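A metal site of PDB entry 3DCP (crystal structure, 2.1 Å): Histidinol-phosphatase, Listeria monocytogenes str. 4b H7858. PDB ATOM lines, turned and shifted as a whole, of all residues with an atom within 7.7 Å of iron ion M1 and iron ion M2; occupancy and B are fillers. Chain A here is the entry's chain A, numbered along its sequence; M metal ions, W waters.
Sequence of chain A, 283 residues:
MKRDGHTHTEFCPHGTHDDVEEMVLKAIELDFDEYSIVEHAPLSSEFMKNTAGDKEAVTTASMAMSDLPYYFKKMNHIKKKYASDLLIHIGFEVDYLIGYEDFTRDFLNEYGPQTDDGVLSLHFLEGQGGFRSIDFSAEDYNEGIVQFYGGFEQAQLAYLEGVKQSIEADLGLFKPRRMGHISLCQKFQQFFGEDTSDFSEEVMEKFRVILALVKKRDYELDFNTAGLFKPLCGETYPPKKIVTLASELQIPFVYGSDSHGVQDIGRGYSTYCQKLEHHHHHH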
ATOM      1  N   HIS A   6      10.782  11.905   9.422  1.00  0.00           N
ATOM      2  CA  HIS A   6      10.992  11.191   8.172  1.00  0.00           C
ATOM      3  C   HIS A   6      12.448  11.218   7.723  1.00  0.00           C
ATOM      4  O   HIS A   6      12.885  12.170   7.072  1.00  0.00           O
ATOM      5  CB  HIS A   6      10.064  11.797   7.108  1.00  0.00           C
ATOM      6  CG  HIS A   6       9.865  10.940   5.896  1.00  0.00           C
ATOM      7  ND1 HIS A   6       8.767  11.081   5.069  1.00  0.00           N
ATOM      8  CD2 HIS A   6      10.623   9.954   5.355  1.00  0.00           C
ATOM      9  CE1 HIS A   6       8.863  10.210   4.075  1.00  0.00           C
ATOM     10  NE2 HIS A   6       9.974   9.522   4.229  1.00  0.00           N
ATOM     11  N   THR A   7      13.201  10.189   8.093  1.00  0.00           N
ATOM     12  CA  THR A   7      14.613  10.107   7.697  1.00  0.00           C
ATOM     13  C   THR A   7      14.985   8.700   7.256  1.00  0.00           C
ATOM     14  O   THR A   7      14.326   7.719   7.615  1.00  0.00           O
ATOM     15  CB  THR A   7      15.557  10.528   8.830  1.00  0.00           C
ATOM     16  OG1 THR A   7      15.548   9.513   9.841  1.00  0.00           O
ATOM     17  CG2 THR A   7      15.111  11.873   9.425  1.00  0.00           C
ATOM     18  N   HIS A   8      16.063   8.590   6.486  1.00  0.00           N
ATOM     19  CA  HIS A   8      16.512   7.307   5.988  1.00  0.00           C
ATOM     20  C   HIS A   8      17.946   6.972   6.408  1.00  0.00           C
ATOM     21  O   HIS A   8      18.603   7.785   7.063  1.00  0.00           O
ATOM     22  CB  HIS A   8      16.336   7.275   4.475  1.00  0.00           C
ATOM     23  CG  HIS A   8      14.907   7.250   4.054  1.00  0.00           C
ATOM     24  ND1 HIS A   8      14.158   6.092   4.003  1.00  0.00           N
ATOM     25  CD2 HIS A   8      14.048   8.257   3.744  1.00  0.00           C
ATOM     26  CE1 HIS A   8      12.918   6.376   3.664  1.00  0.00           C
ATOM     27  NE2 HIS A   8      12.820   7.686   3.505  1.00  0.00           N
ATOM     28  N   CYS A  12      19.210   2.057   2.848  1.00  0.00           N
ATOM     29  CA  CYS A  12      18.433   2.462   1.681  1.00  0.00           C
ATOM     30  C   CYS A  12      19.300   2.332   0.442  1.00  0.00           C
ATOM     31  O   CYS A  12      20.298   3.031   0.294  1.00  0.00           O
ATOM     32  CB  CYS A  12      17.957   3.912   1.832  1.00  0.00           C
ATOM     33  SG  CYS A  12      17.045   4.502   0.391  1.00  0.00           S
ATOM     34  N   HIS A  14      19.000   3.377  -2.580  1.00  0.00           N
ATOM     35  CA  HIS A  14      19.172   4.575  -3.387  1.00  0.00           C
ATOM     36  C   HIS A  14      19.590   5.796  -2.582  1.00  0.00           C
ATOM     37  O   HIS A  14      19.564   6.925  -3.087  1.00  0.00           O
ATOM     38  CB  HIS A  14      17.890   4.905  -4.149  1.00  0.00           C
ATOM     39  CG  HIS A  14      16.669   4.966  -3.279  1.00  0.00           C
ATOM     40  ND1 HIS A  14      15.958   3.837  -2.934  1.00  0.00           N
ATOM     41  CD2 HIS A  14      16.055   6.003  -2.668  1.00  0.00           C
ATOM     42  CE1 HIS A  14      14.961   4.182  -2.139  1.00  0.00           C
ATOM     43  NE2 HIS A  14      14.997   5.489  -1.958  1.00  0.00           N
ATOM     44  N   VAL A  38      12.615   5.992   9.569  1.00  0.00           N
ATOM     45  CA  VAL A  38      11.572   5.243   8.908  1.00  0.00           C
ATOM     46  C   VAL A  38      12.081   4.779   7.546  1.00  0.00           C
ATOM     47  O   VAL A  38      11.734   5.328   6.504  1.00  0.00           O
ATOM     48  CB  VAL A  38      10.312   6.096   8.749  1.00  0.00           C
ATOM     49  CG1 VAL A  38       9.625   6.253  10.106  1.00  0.00           C
ATOM     50  CG2 VAL A  38      10.689   7.486   8.216  1.00  0.00           C
ATOM     51  N   GLU A  39      12.938   3.766   7.578  1.00  0.00           N
ATOM     52  CA  GLU A  39      13.516   3.241   6.369  1.00  0.00           C
ATOM     53  C   GLU A  39      12.452   2.538   5.510  1.00  0.00           C
ATOM     54  O   GLU A  39      11.428   2.094   6.013  1.00  0.00           O
ATOM     55  CB  GLU A  39      14.638   2.267   6.699  1.00  0.00           C
ATOM     56  CG  GLU A  39      15.416   1.861   5.494  1.00  0.00           C
ATOM     57  CD  GLU A  39      15.918   3.078   4.739  1.00  0.00           C
ATOM     58  OE1 GLU A  39      16.928   3.674   5.184  1.00  0.00           O
ATOM     59  OE2 GLU A  39      15.297   3.441   3.739  1.00  0.00           O
ATOM     60  N   HIS A  40      12.717   2.464   4.206  1.00  0.00           N
ATOM     61  CA  HIS A  40      11.794   1.803   3.298  1.00  0.00           C
ATOM     62  C   HIS A  40      11.601   0.322   3.619  1.00  0.00           C
ATOM     63  O   HIS A  40      12.573  -0.442   3.705  1.00  0.00           O
ATOM     64  CB  HIS A  40      12.295   1.922   1.866  1.00  0.00           C
ATOM     65  CG  HIS A  40      12.211   3.307   1.320  1.00  0.00           C
ATOM     66  ND1 HIS A  40      11.013   3.881   0.938  1.00  0.00           N
ATOM     67  CD2 HIS A  40      13.157   4.242   1.093  1.00  0.00           C
ATOM     68  CE1 HIS A  40      11.222   5.106   0.505  1.00  0.00           C
ATOM     69  NE2 HIS A  40      12.524   5.359   0.593  1.00  0.00           N
ATOM     70  N   GLU A  93       8.963   3.469   6.377  1.00  0.00           N
ATOM     71  CA  GLU A  93       8.156   4.256   5.460  1.00  0.00           C
ATOM     72  C   GLU A  93       7.524   3.085   4.701  1.00  0.00           C
ATOM     73  O   GLU A  93       8.180   2.439   3.891  1.00  0.00           O
ATOM     74  CB  GLU A  93       8.975   5.089   4.497  1.00  0.00           C
ATOM     75  CG  GLU A  93       8.114   5.628   3.371  1.00  0.00           C
ATOM     76  CD  GLU A  93       8.761   6.752   2.604  1.00  0.00           C
ATOM     77  OE1 GLU A  93       9.993   6.778   2.522  1.00  0.00           O
ATOM     78  OE2 GLU A  93       8.020   7.601   2.066  1.00  0.00           O
ATOM     79  N   VAL A  94       6.273   2.778   5.023  1.00  0.00           N
ATOM     80  CA  VAL A  94       5.600   1.655   4.394  1.00  0.00           C
ATOM     81  C   VAL A  94       4.925   2.012   3.090  1.00  0.00           C
ATOM     82  O   VAL A  94       4.133   2.947   3.025  1.00  0.00           O
ATOM     83  CB  VAL A  94       4.556   1.057   5.351  1.00  0.00           C
ATOM     84  CG1 VAL A  94       3.877  -0.142   4.695  1.00  0.00           C
ATOM     85  CG2 VAL A  94       5.221   0.653   6.670  1.00  0.00           C
ATOM     86  N   ASP A  95       5.261   1.260   2.049  1.00  0.00           N
ATOM     87  CA  ASP A  95       4.673   1.453   0.724  1.00  0.00           C
ATOM     88  C   ASP A  95       3.245   0.945   0.696  1.00  0.00           C
ATOM     89  O   ASP A  95       2.988  -0.213   1.063  1.00  0.00           O
ATOM     90  CB  ASP A  95       5.465   0.684  -0.332  1.00  0.00           C
ATOM     91  CG  ASP A  95       6.510   1.517  -1.014  1.00  0.00           C
ATOM     92  OD1 ASP A  95       6.153   2.301  -1.921  1.00  0.00           O
ATOM     93  OD2 ASP A  95       7.700   1.382  -0.636  1.00  0.00           O
ATOM     94  N   VAL A 119       5.353   5.817   8.600  1.00  0.00           N
ATOM     95  CA  VAL A 119       4.756   6.630   7.548  1.00  0.00           C
ATOM     96  C   VAL A 119       4.251   5.676   6.482  1.00  0.00           C
ATOM     97  O   VAL A 119       4.916   4.682   6.165  1.00  0.00           O
ATOM     98  CB  VAL A 119       5.805   7.577   6.908  1.00  0.00           C
ATOM     99  CG1 VAL A 119       5.167   8.391   5.789  1.00  0.00           C
ATOM    100  CG2 VAL A 119       6.407   8.504   7.961  1.00  0.00           C
ATOM    101  N   LEU A 120       3.061   5.955   5.953  1.00  0.00           N
ATOM    102  CA  LEU A 120       2.472   5.136   4.896  1.00  0.00           C
ATOM    103  C   LEU A 120       2.531   6.011   3.647  1.00  0.00           C
ATOM    104  O   LEU A 120       1.934   7.088   3.614  1.00  0.00           O
ATOM    105  CB  LEU A 120       1.022   4.807   5.217  1.00  0.00           C
ATOM    106  CG  LEU A 120       0.425   3.458   4.800  1.00  0.00           C
ATOM    107  CD1 LEU A 120      -1.082   3.638   4.575  1.00  0.00           C
ATOM    108  CD2 LEU A 120       1.092   2.918   3.550  1.00  0.00           C
ATOM    109  N   SER A 121       3.237   5.554   2.621  1.00  0.00           N
ATOM    110  CA  SER A 121       3.401   6.341   1.402  1.00  0.00           C
ATOM    111  C   SER A 121       3.014   5.656   0.099  1.00  0.00           C
ATOM    112  O   SER A 121       3.182   4.437  -0.057  1.00  0.00           O
ATOM    113  CB  SER A 121       4.861   6.811   1.280  1.00  0.00           C
ATOM    114  OG  SER A 121       5.276   7.578   2.402  1.00  0.00           O
ATOM    115  N   LEU A 122       2.533   6.438  -0.849  1.00  0.00           N
ATOM    116  CA  LEU A 122       2.162   5.925  -2.154  1.00  0.00           C
ATOM    117  C   LEU A 122       3.318   6.278  -3.105  1.00  0.00           C
ATOM    118  O   LEU A 122       3.592   7.465  -3.323  1.00  0.00           O
ATOM    119  CB  LEU A 122       0.870   6.583  -2.620  1.00  0.00           C
ATOM    120  CG  LEU A 122      -0.085   5.819  -3.556  1.00  0.00           C
ATOM    121  CD1 LEU A 122      -0.669   6.790  -4.572  1.00  0.00           C
ATOM    122  CD2 LEU A 122       0.649   4.674  -4.240  1.00  0.00           C
ATOM    123  N   HIS A 123       3.977   5.260  -3.675  1.00  0.00           N
ATOM    124  CA  HIS A 123       5.102   5.467  -4.594  1.00  0.00           C
ATOM    125  C   HIS A 123       4.887   4.825  -5.966  1.00  0.00           C
ATOM    126  O   HIS A 123       5.563   5.182  -6.939  1.00  0.00           O
ATOM    127  CB  HIS A 123       6.401   4.885  -4.016  1.00  0.00           C
ATOM    128  CG  HIS A 123       6.881   5.574  -2.779  1.00  0.00           C
ATOM    129  ND1 HIS A 123       7.148   4.887  -1.611  1.00  0.00           N
ATOM    130  CD2 HIS A 123       7.132   6.882  -2.520  1.00  0.00           C
ATOM    131  CE1 HIS A 123       7.560   5.742  -0.692  1.00  0.00           C
ATOM    132  NE2 HIS A 123       7.553   6.961  -1.217  1.00  0.00           N
ATOM    133  N   ASP A 135       7.900   8.530  -8.495  1.00  0.00           N
ATOM    134  CA  ASP A 135       9.024   9.428  -8.222  1.00  0.00           C
ATOM    135  C   ASP A 135      10.443   9.088  -8.719  1.00  0.00           C
ATOM    136  O   ASP A 135      11.402   9.742  -8.312  1.00  0.00           O
ATOM    137  CB  ASP A 135       9.089   9.654  -6.701  1.00  0.00           C
ATOM    138  CG  ASP A 135       9.317   8.366  -5.941  1.00  0.00           C
ATOM    139  OD1 ASP A 135       9.291   7.301  -6.576  1.00  0.00           O
ATOM    140  OD2 ASP A 135       9.525   8.408  -4.709  1.00  0.00           O
ATOM    141  N   GLY A 180       2.511   9.820   4.127  1.00  0.00           N
ATOM    142  CA  GLY A 180       3.672  10.432   3.503  1.00  0.00           C
ATOM    143  C   GLY A 180       3.435  11.353   2.303  1.00  0.00           C
ATOM    144  O   GLY A 180       2.592  11.064   1.459  1.00  0.00           O
ATOM    145  N   HIS A 181       4.193  12.457   2.260  1.00  0.00           N
ATOM    146  CA  HIS A 181       4.161  13.428   1.157  1.00  0.00           C
ATOM    147  C   HIS A 181       2.966  13.263   0.214  1.00  0.00           C
ATOM    148  O   HIS A 181       3.122  12.770  -0.896  1.00  0.00           O
ATOM    149  CB  HIS A 181       5.457  13.285   0.348  1.00  0.00           C
ATOM    150  CG  HIS A 181       5.836  11.862   0.061  1.00  0.00           C
ATOM    151  ND1 HIS A 181       4.987  10.964  -0.543  1.00  0.00           N
ATOM    152  CD2 HIS A 181       6.980  11.183   0.317  1.00  0.00           C
ATOM    153  CE1 HIS A 181       5.584   9.791  -0.661  1.00  0.00           C
ATOM    154  NE2 HIS A 181       6.794   9.893  -0.144  1.00  0.00           N
ATOM    155  N   LEU A 184       3.016  13.956  -3.972  1.00  0.00           N
ATOM    156  CA  LEU A 184       4.178  13.428  -4.661  1.00  0.00           C
ATOM    157  C   LEU A 184       4.034  13.499  -6.178  1.00  0.00           C
ATOM    158  O   LEU A 184       5.023  13.449  -6.911  1.00  0.00           O
ATOM    159  CB  LEU A 184       4.434  11.987  -4.240  1.00  0.00           C
ATOM    160  CG  LEU A 184       5.780  11.404  -4.712  1.00  0.00           C
ATOM    161  CD1 LEU A 184       6.930  12.131  -3.998  1.00  0.00           C
ATOM    162  CD2 LEU A 184       5.812   9.923  -4.406  1.00  0.00           C
ATOM    163  N   ASP A 222       2.574  14.030   6.851  1.00  0.00           N
ATOM    164  CA  ASP A 222       4.023  14.205   6.710  1.00  0.00           C
ATOM    165  C   ASP A 222       4.239  15.518   5.948  1.00  0.00           C
ATOM    166  O   ASP A 222       3.857  15.618   4.786  1.00  0.00           O
ATOM    167  CB  ASP A 222       4.547  12.991   5.923  1.00  0.00           C
ATOM    168  CG  ASP A 222       5.986  13.129   5.448  1.00  0.00           C
ATOM    169  OD1 ASP A 222       6.862  13.528   6.238  1.00  0.00           O
ATOM    170  OD2 ASP A 222       6.251  12.767   4.274  1.00  0.00           O
ATOM    171  N   ASN A 224       6.542  17.180   4.236  1.00  0.00           N
ATOM    172  CA  ASN A 224       7.792  16.823   3.593  1.00  0.00           C
ATOM    173  C   ASN A 224       8.438  17.945   2.773  1.00  0.00           C
ATOM    174  O   ASN A 224       7.865  18.440   1.801  1.00  0.00           O
ATOM    175  CB  ASN A 224       7.506  15.601   2.713  1.00  0.00           C
ATOM    176  CG  ASN A 224       8.753  14.839   2.340  1.00  0.00           C
ATOM    177  OD1 ASN A 224       9.690  15.404   1.768  1.00  0.00           O
ATOM    178  ND2 ASN A 224       8.763  13.541   2.635  1.00  0.00           N
ATOM    179  N   ALA A 226      11.365  17.653   1.157  1.00  0.00           N
ATOM    180  CA  ALA A 226      12.237  17.109   0.122  1.00  0.00           C
ATOM    181  C   ALA A 226      11.991  17.802  -1.224  1.00  0.00           C
ATOM    182  O   ALA A 226      12.931  18.051  -1.972  1.00  0.00           O
ATOM    183  CB  ALA A 226      12.006  15.603  -0.026  1.00  0.00           C
ATOM    184  N   SER A 257      12.073  15.740   6.751  1.00  0.00           N
ATOM    185  CA  SER A 257      13.150  16.154   5.859  1.00  0.00           C
ATOM    186  C   SER A 257      13.383  15.114   4.772  1.00  0.00           C
ATOM    187  O   SER A 257      13.994  15.409   3.740  1.00  0.00           O
ATOM    188  CB  SER A 257      14.445  16.312   6.646  1.00  0.00           C
ATOM    189  OG  SER A 257      14.942  15.043   7.050  1.00  0.00           O
ATOM    190  N   ASP A 258      12.909  13.899   5.008  1.00  0.00           N
ATOM    191  CA  ASP A 258      13.091  12.809   4.059  1.00  0.00           C
ATOM    192  C   ASP A 258      14.589  12.694   3.732  1.00  0.00           C
ATOM    193  O   ASP A 258      14.965  12.417   2.587  1.00  0.00           O
ATOM    194  CB  ASP A 258      12.306  13.086   2.771  1.00  0.00           C
ATOM    195  CG  ASP A 258      11.744  11.808   2.170  1.00  0.00           C
ATOM    196  OD1 ASP A 258      12.344  10.740   2.355  1.00  0.00           O
ATOM    197  OD2 ASP A 258      10.694  11.883   1.493  1.00  0.00           O
ATOM    198  N   SER A 259      15.433  12.890   4.735  1.00  0.00           N
ATOM    199  CA  SER A 259      16.883  12.840   4.556  1.00  0.00           C
ATOM    200  C   SER A 259      17.416  11.465   4.169  1.00  0.00           C
ATOM    201  O   SER A 259      17.046  10.441   4.768  1.00  0.00           O
ATOM    202  CB  SER A 259      17.603  13.312   5.829  1.00  0.00           C
ATOM    203  OG  SER A 259      17.344  14.676   6.114  1.00  0.00           O
ATOM    204  N   HIS A 260      18.284  11.432   3.167  1.00  0.00           N
ATOM    205  CA  HIS A 260      18.919  10.202   2.712  1.00  0.00           C
ATOM    206  C   HIS A 260      20.423  10.344   2.860  1.00  0.00           C
ATOM    207  O   HIS A 260      21.200   9.541   2.344  1.00  0.00           O
ATOM    208  CB  HIS A 260      18.576   9.916   1.245  1.00  0.00           C
ATOM    209  CG  HIS A 260      17.138   9.557   1.025  1.00  0.00           C
ATOM    210  ND1 HIS A 260      16.116  10.467   1.221  1.00  0.00           N
ATOM    211  CD2 HIS A 260      16.550   8.395   0.686  1.00  0.00           C
ATOM    212  CE1 HIS A 260      14.955   9.874   1.001  1.00  0.00           C
ATOM    213  NE2 HIS A 260      15.186   8.616   0.677  1.00  0.00           N
HETATM  214 FE    FE M   1       8.585   8.418   0.003  1.00  0.00          FE
HETATM  215 FE    FE M   2      11.109   8.740   2.480  1.00  0.00          FE
HETATM  216 ZN    ZN M   3      14.108   6.847  -0.263  1.00  0.00          ZN
HETATM  217  O   HOH W   1      11.917   8.566  -0.747  1.00  0.00           O
HETATM  218  O   HOH W   2       8.864   9.708  -2.050  1.00  0.00           O
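ND1 of His 123 is in hydrogen-bond range of OD1 of Asp 95.
A ring nitrogen (ND1) of His 6 sits at hydrogen-bond distance from the side-chain amide nitrogen (ND2) of Asn 224, 3.5 Å away.
The backbone NH (N) of His 8 sits at hydrogen-bond distance from the backbone carbonyl oxygen (O) of Ser 259, at 2.7 Å.
A ring nitrogen (ND1) of His 8 is in hydrogen-bond range of the side-chain carboxylate (OE2) of Glu 39.
OE2 of Glu 93 sits close to OG of Ser 121 (2.8 Å).
The backbone NH (N) of Glu 93 lies within hydrogen-bond range of the backbone carbonyl oxygen (O) of Val 38, 3.3 Å away.
N of Glu 93 lies within hydrogen-bond range of O of Glu 39, 2.8 Å away.
O of Asp 258 sits at hydrogen-bond distance from ND1 of His 260 (2.6 Å).
Iron ion M1 is bound by NE2 of His 123 (2.2 Å), OE2 of Glu 93 (2.3 Å), NE2 of His 181 (2.3 Å) and water W2 (2.4 Å).
The nearest printed residue that does not touch iron ion M2 is His 40 (4.1 Å).
Iron ion M2 is bound by a ring nitrogen (NE2) of His 6 (2.2 Å), a ring nitrogen (NE2) of His 8 (2.3 Å), the side-chain carboxylate of Glu 93 (2.3 Å) and the side-chain carboxylate of Asp 258 (2.4 Å).
Three residues have an atom within 4 Å of iron ion M1: Glu 93, His 123 and His 181.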
